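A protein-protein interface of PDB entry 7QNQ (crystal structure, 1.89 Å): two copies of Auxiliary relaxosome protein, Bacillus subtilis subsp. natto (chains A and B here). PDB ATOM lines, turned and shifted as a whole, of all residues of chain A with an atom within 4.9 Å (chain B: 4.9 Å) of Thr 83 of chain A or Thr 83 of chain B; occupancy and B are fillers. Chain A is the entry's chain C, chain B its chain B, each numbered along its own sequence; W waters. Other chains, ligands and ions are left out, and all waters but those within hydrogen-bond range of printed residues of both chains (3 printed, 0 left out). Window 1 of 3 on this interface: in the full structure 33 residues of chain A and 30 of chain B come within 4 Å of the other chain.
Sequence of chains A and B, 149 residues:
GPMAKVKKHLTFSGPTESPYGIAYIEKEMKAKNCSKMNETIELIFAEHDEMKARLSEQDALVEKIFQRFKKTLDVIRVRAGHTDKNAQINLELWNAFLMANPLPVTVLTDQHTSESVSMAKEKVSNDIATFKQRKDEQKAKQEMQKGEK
The backbone carbonyl oxygen of Arg 79 of chain B is in hydrogen-bond range of the side-chain hydroxyl of Thr 83 of chain B (2.9 Å). O of His 82 of chain B is in hydrogen-bond range of ND2 of Asn 86 of chain B. O of Arg 79 of chain A sits at hydrogen-bond distance from OG1 of Thr 83 of chain A (2.9 Å).
Ala 80 of chain A touches Arg 79 of chain B (O to CB, 3.9 Å). Gly 81 of chain A touches Arg 79 of chain B (CA to CD, 3.6 Å). CG2 of Thr 83 of chain B touches CG2 of Thr 83 of chain A (3.5 Å). CG of Arg 79 of chain B touches OD2 of Asp 84 of chain A, at 3.9 Å. OG1 of Thr 83 of chain B touches CA of Asp 84 of chain A (3.4 Å). Ala 87 of chain A touches Asn 86 of chain B (CB to CB, 3.9 Å).
Of chain B, only Thr 83 comes within 4 Å of Thr 83 of chain A. Of chain A, only Thr 83 and Asp 84 come within 4 Å of Thr 83 of chain B. Of the printed residues of chain B, Gly 81 of chain A touches Arg 79. Of the printed residues of chain B, Ala 80 of chain A touches Arg 79. Of the printed residues of chain A, Arg 79 of chain B touches Ala 80 (3.9 Å), Gly 81 (3.6 Å) and Asp 84 (3.9 Å). Printed residues of chain B within 4 Å of Ala 87 of chain A: Asn 86 (3.9 Å). Of the printed residues of chain A, Asn 86 of chain B touches Ala 87 (3.9 Å). The nearest residue of chain A that does not touch Thr 83 of chain B is Ala 80 of chain A (4.5 Å). The nearest printed residue of chain A that does not touch Arg 79 of chain B is His 82 of chain A (5.7 Å).
Hydrophobic or aromatic side chains of chain A within 4 Å of the printed part of chain B: Ala 80 and Ala 87. Printed residues of chain B that touch a printed residue of chain A: Arg 79, Thr 83 and Asn 86. Among the printed residues, 6 pairs touch across the chains. Among the printed residues, no Asp or Glu carboxylate lies within 4 Å of a Lys or Arg side-chain nitrogen of the other chain.
Thr 83 of chain B touches its own counterpart, Thr 83 of chain A. Asp 84 of chain A touches Arg 79 of chain B, but with the chains exchanged Arg 79 of chain A does not touch Asp 84 of chain B (10.7 Å). Asp 84 of chain A touches Thr 83 of chain B, but with the chains exchanged Thr 83 of chain A does not touch Asp 84 of chain B (7.2 Å). Ala 87 of chain A touches Asn 86 of chain B, but with the chains exchanged Asn 86 of chain A does not touch Ala 87 of chain B (8.8 Å). Positions printed for both chains: 79, 80, 81, 82, 83, 84, 85, 86 and 87. Of the 6 pairs that touch across the chains among the printed residues, 1 has its exchanged pair printed and touching as well.
Water W1 bridges the side-chain carboxylate of Asp 84 of chain A and the side-chain amide nitrogen of Asn 86 of chain B. Water W3 lies within hydrogen-bond range of O of Ala 80 of chain A (2.6 Å), OG1 of Thr 83 of chain B (2.6 Å) and O of Arg 79 of chain B (3.4 Å). Water W2 bridges O of Ala 87 of chain A (2.7 Å) and O of Asn 86 of chain B (3.4 Å).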
ATOM      1  N   ARG A  79     -22.263  13.271 -29.874  1.00  0.00           N
ATOM      2  CA  ARG A  79     -21.464  14.457 -29.574  1.00  0.00           C
ATOM      3  C   ARG A  79     -20.204  14.112 -28.805  1.00  0.00           C
ATOM      4  O   ARG A  79     -19.142  14.684 -29.067  1.00  0.00           O
ATOM      5  CB  ARG A  79     -22.274  15.475 -28.785  1.00  0.00           C
ATOM      6  CG  ARG A  79     -23.106  16.357 -29.641  1.00  0.00           C
ATOM      7  CD  ARG A  79     -24.023  17.143 -28.777  1.00  0.00           C
ATOM      8  NE  ARG A  79     -24.961  17.897 -29.585  1.00  0.00           N
ATOM      9  CZ  ARG A  79     -26.041  18.476 -29.086  1.00  0.00           C
ATOM     10  NH1 ARG A  79     -26.323  18.324 -27.795  1.00  0.00           N
ATOM     11  NH2 ARG A  79     -26.856  19.154 -29.883  1.00  0.00           N
ATOM     12  N   ALA A  80     -20.306  13.205 -27.830  1.00  0.00           N
ATOM     13  CA  ALA A  80     -19.116  12.796 -27.091  1.00  0.00           C
ATOM     14  C   ALA A  80     -18.085  12.182 -28.026  1.00  0.00           C
ATOM     15  O   ALA A  80     -16.878  12.332 -27.810  1.00  0.00           O
ATOM     16  CB  ALA A  80     -19.486  11.819 -25.974  1.00  0.00           C
ATOM     17  N   GLY A  81     -18.541  11.459 -29.052  1.00  0.00           N
ATOM     18  CA  GLY A  81     -17.614  10.908 -30.028  1.00  0.00           C
ATOM     19  C   GLY A  81     -16.936  11.980 -30.865  1.00  0.00           C
ATOM     20  O   GLY A  81     -15.720  11.942 -31.067  1.00  0.00           O
ATOM     21  N   HIS A  82     -17.705  12.962 -31.348  1.00  0.00           N
ATOM     22  CA  HIS A  82     -17.100  14.045 -32.125  1.00  0.00           C
ATOM     23  C   HIS A  82     -16.151  14.875 -31.270  1.00  0.00           C
ATOM     24  O   HIS A  82     -15.077  15.279 -31.735  1.00  0.00           O
ATOM     25  CB  HIS A  82     -18.188  14.948 -32.713  1.00  0.00           C
ATOM     26  CG  HIS A  82     -18.939  14.334 -33.852  1.00  0.00           C
ATOM     27  ND1 HIS A  82     -20.312  14.396 -33.958  1.00  0.00           N
ATOM     28  CD2 HIS A  82     -18.509  13.648 -34.938  1.00  0.00           C
ATOM     29  CE1 HIS A  82     -20.696  13.771 -35.057  1.00  0.00           C
ATOM     30  NE2 HIS A  82     -19.622  13.306 -35.668  1.00  0.00           N
ATOM     31  N   THR A  83     -16.529  15.139 -30.017  1.00  0.00           N
ATOM     32  CA  THR A  83     -15.666  15.896 -29.116  1.00  0.00           C
ATOM     33  C   THR A  83     -14.379  15.141 -28.796  1.00  0.00           C
ATOM     34  O   THR A  83     -13.302  15.742 -28.711  1.00  0.00           O
ATOM     35  CB  THR A  83     -16.425  16.223 -27.835  1.00  0.00           C
ATOM     36  OG1 THR A  83     -17.591  16.987 -28.166  1.00  0.00           O
ATOM     37  CG2 THR A  83     -15.562  17.048 -26.927  1.00  0.00           C
ATOM     38  N   ASP A  84     -14.482  13.832 -28.568  1.00  0.00           N
ATOM     39  CA  ASP A  84     -13.300  13.019 -28.306  1.00  0.00           C
ATOM     40  C   ASP A  84     -12.352  13.035 -29.501  1.00  0.00           C
ATOM     41  O   ASP A  84     -11.138  13.217 -29.341  1.00  0.00           O
ATOM     42  CB  ASP A  84     -13.757  11.598 -27.950  1.00  0.00           C
ATOM     43  CG  ASP A  84     -12.609  10.636 -27.687  1.00  0.00           C
ATOM     44  OD1 ASP A  84     -11.517  11.071 -27.278  1.00  0.00           O
ATOM     45  OD2 ASP A  84     -12.839   9.414 -27.852  1.00  0.00           O
ATOM     46  N   LYS A  85     -12.891  12.886 -30.714  1.00  0.00           N
ATOM     47  CA  LYS A  85     -12.048  12.959 -31.902  1.00  0.00           C
ATOM     48  C   LYS A  85     -11.376  14.324 -32.026  1.00  0.00           C
ATOM     49  O   LYS A  85     -10.179  14.410 -32.321  1.00  0.00           O
ATOM     50  CB  LYS A  85     -12.867  12.642 -33.151  1.00  0.00           C
ATOM     51  CG  LYS A  85     -12.077  12.754 -34.434  1.00  0.00           C
ATOM     52  CD  LYS A  85     -12.950  12.570 -35.672  1.00  0.00           C
ATOM     53  CE  LYS A  85     -12.080  12.505 -36.929  1.00  0.00           C
ATOM     54  NZ  LYS A  85     -12.745  11.824 -38.074  1.00  0.00           N
ATOM     55  N   ASN A  86     -12.126  15.407 -31.796  1.00  0.00           N
ATOM     56  CA  ASN A  86     -11.542  16.739 -31.933  1.00  0.00           C
ATOM     57  C   ASN A  86     -10.490  16.999 -30.863  1.00  0.00           C
ATOM     58  O   ASN A  86      -9.478  17.656 -31.130  1.00  0.00           O
ATOM     59  CB  ASN A  86     -12.630  17.810 -31.864  1.00  0.00           C
ATOM     60  CG  ASN A  86     -13.462  17.880 -33.137  1.00  0.00           C
ATOM     61  OD1 ASN A  86     -12.979  17.569 -34.228  1.00  0.00           O
ATOM     62  ND2 ASN A  86     -14.704  18.330 -33.009  1.00  0.00           N
ATOM     63  N   ALA A  87     -10.698  16.482 -29.648  1.00  0.00           N
ATOM     64  CA  ALA A  87      -9.678  16.635 -28.613  1.00  0.00           C
ATOM     65  C   ALA A  87      -8.392  15.903 -28.992  1.00  0.00           C
ATOM     66  O   ALA A  87      -7.287  16.365 -28.674  1.00  0.00           O
ATOM     67  CB  ALA A  87     -10.208  16.141 -27.263  1.00  0.00           C
ATOM     68  N   ARG B  79     -15.707   8.146 -23.385  1.00  0.00           N
ATOM     69  CA  ARG B  79     -15.388   9.244 -24.294  1.00  0.00           C
ATOM     70  C   ARG B  79     -15.263  10.563 -23.543  1.00  0.00           C
ATOM     71  O   ARG B  79     -14.309  11.320 -23.752  1.00  0.00           O
ATOM     72  CB  ARG B  79     -16.459   9.350 -25.377  1.00  0.00           C
ATOM     73  CG  ARG B  79     -16.299   8.327 -26.482  1.00  0.00           C
ATOM     74  CD  ARG B  79     -17.459   8.388 -27.456  1.00  0.00           C
ATOM     75  NE  ARG B  79     -17.363   7.334 -28.458  1.00  0.00           N
ATOM     76  CZ  ARG B  79     -18.282   7.092 -29.386  1.00  0.00           C
ATOM     77  NH1 ARG B  79     -19.392   7.823 -29.434  1.00  0.00           N
ATOM     78  NH2 ARG B  79     -18.094   6.113 -30.260  1.00  0.00           N
ATOM     79  N   ALA B  80     -16.206  10.842 -22.644  1.00  0.00           N
ATOM     80  CA  ALA B  80     -16.127  12.059 -21.837  1.00  0.00           C
ATOM     81  C   ALA B  80     -14.887  12.061 -20.950  1.00  0.00           C
ATOM     82  O   ALA B  80     -14.312  13.120 -20.680  1.00  0.00           O
ATOM     83  CB  ALA B  80     -17.383  12.203 -20.982  1.00  0.00           C
ATOM     84  N   GLY B  81     -14.491  10.890 -20.447  1.00  0.00           N
ATOM     85  CA  GLY B  81     -13.310  10.824 -19.602  1.00  0.00           C
ATOM     86  C   GLY B  81     -12.029  11.169 -20.336  1.00  0.00           C
ATOM     87  O   GLY B  81     -11.197  11.924 -19.828  1.00  0.00           O
ATOM     88  N   HIS B  82     -11.842  10.613 -21.530  1.00  0.00           N
ATOM     89  CA  HIS B  82     -10.656  10.956 -22.305  1.00  0.00           C
ATOM     90  C   HIS B  82     -10.698  12.406 -22.761  1.00  0.00           C
ATOM     91  O   HIS B  82      -9.657  13.067 -22.835  1.00  0.00           O
ATOM     92  CB  HIS B  82     -10.505   9.993 -23.477  1.00  0.00           C
ATOM     93  CG  HIS B  82     -10.057   8.633 -23.047  1.00  0.00           C
ATOM     94  ND1 HIS B  82      -8.821   8.405 -22.484  1.00  0.00           N
ATOM     95  CD2 HIS B  82     -10.701   7.444 -23.034  1.00  0.00           C
ATOM     96  CE1 HIS B  82      -8.710   7.127 -22.172  1.00  0.00           C
ATOM     97  NE2 HIS B  82      -9.839   6.521 -22.494  1.00  0.00           N
ATOM     98  N   THR B  83     -11.887  12.919 -23.085  1.00  0.00           N
ATOM     99  CA  THR B  83     -11.980  14.327 -23.467  1.00  0.00           C
ATOM    100  C   THR B  83     -11.549  15.231 -22.318  1.00  0.00           C
ATOM    101  O   THR B  83     -10.784  16.182 -22.517  1.00  0.00           O
ATOM    102  CB  THR B  83     -13.410  14.649 -23.897  1.00  0.00           C
ATOM    103  OG1 THR B  83     -13.745  13.848 -25.034  1.00  0.00           O
ATOM    104  CG2 THR B  83     -13.573  16.148 -24.238  1.00  0.00           C
ATOM    105  N   ASP B  84     -11.994  14.917 -21.100  1.00  0.00           N
ATOM    106  CA  ASP B  84     -11.611  15.704 -19.930  1.00  0.00           C
ATOM    107  C   ASP B  84     -10.113  15.633 -19.695  1.00  0.00           C
ATOM    108  O   ASP B  84      -9.478  16.640 -19.364  1.00  0.00           O
ATOM    109  CB  ASP B  84     -12.369  15.207 -18.695  1.00  0.00           C
ATOM    110  CG  ASP B  84     -12.056  16.028 -17.442  1.00  0.00           C
ATOM    111  OD1 ASP B  84     -11.635  15.441 -16.417  1.00  0.00           O
ATOM    112  OD2 ASP B  84     -12.194  17.266 -17.497  1.00  0.00           O
ATOM    113  N   LYS B  85      -9.537  14.437 -19.834  1.00  0.00           N
ATOM    114  CA  LYS B  85      -8.096  14.274 -19.691  1.00  0.00           C
ATOM    115  C   LYS B  85      -7.349  15.124 -20.713  1.00  0.00           C
ATOM    116  O   LYS B  85      -6.395  15.831 -20.372  1.00  0.00           O
ATOM    117  CB  LYS B  85      -7.736  12.802 -19.881  1.00  0.00           C
ATOM    118  CG  LYS B  85      -6.239  12.543 -19.891  1.00  0.00           C
ATOM    119  CD  LYS B  85      -5.983  11.134 -20.426  1.00  0.00           C
ATOM    120  CE  LYS B  85      -6.052  11.199 -21.970  1.00  0.00           C
ATOM    121  NZ  LYS B  85      -6.340   9.922 -22.692  1.00  0.00           N
ATOM    122  N   ASN B  86      -7.781  15.075 -21.976  1.00  0.00           N
ATOM    123  CA  ASN B  86      -7.105  15.843 -23.021  1.00  0.00           C
ATOM    124  C   ASN B  86      -7.287  17.341 -22.831  1.00  0.00           C
ATOM    125  O   ASN B  86      -6.388  18.121 -23.162  1.00  0.00           O
ATOM    126  CB  ASN B  86      -7.618  15.419 -24.395  1.00  0.00           C
ATOM    127  CG  ASN B  86      -7.018  14.107 -24.847  1.00  0.00           C
ATOM    128  OD1 ASN B  86      -5.877  13.802 -24.518  1.00  0.00           O
ATOM    129  ND2 ASN B  86      -7.784  13.322 -25.595  1.00  0.00           N
ATOM    130  N   ALA B  87      -8.443  17.761 -22.316  1.00  0.00           N
ATOM    131  CA  ALA B  87      -8.631  19.174 -22.006  1.00  0.00           C
ATOM    132  C   ALA B  87      -7.663  19.627 -20.916  1.00  0.00           C
ATOM    133  O   ALA B  87      -7.156  20.753 -20.954  1.00  0.00           O
ATOM    134  CB  ALA B  87     -10.080  19.430 -21.582  1.00  0.00           C
HETATM  135  O   HOH W   1     -10.303  12.893 -26.276  1.00  0.00           O
HETATM  136  O   HOH W   2      -6.807  18.056 -26.571  1.00  0.00           O
HETATM  137  O   HOH W   3     -16.299  13.411 -25.506  1.00  0.00           O
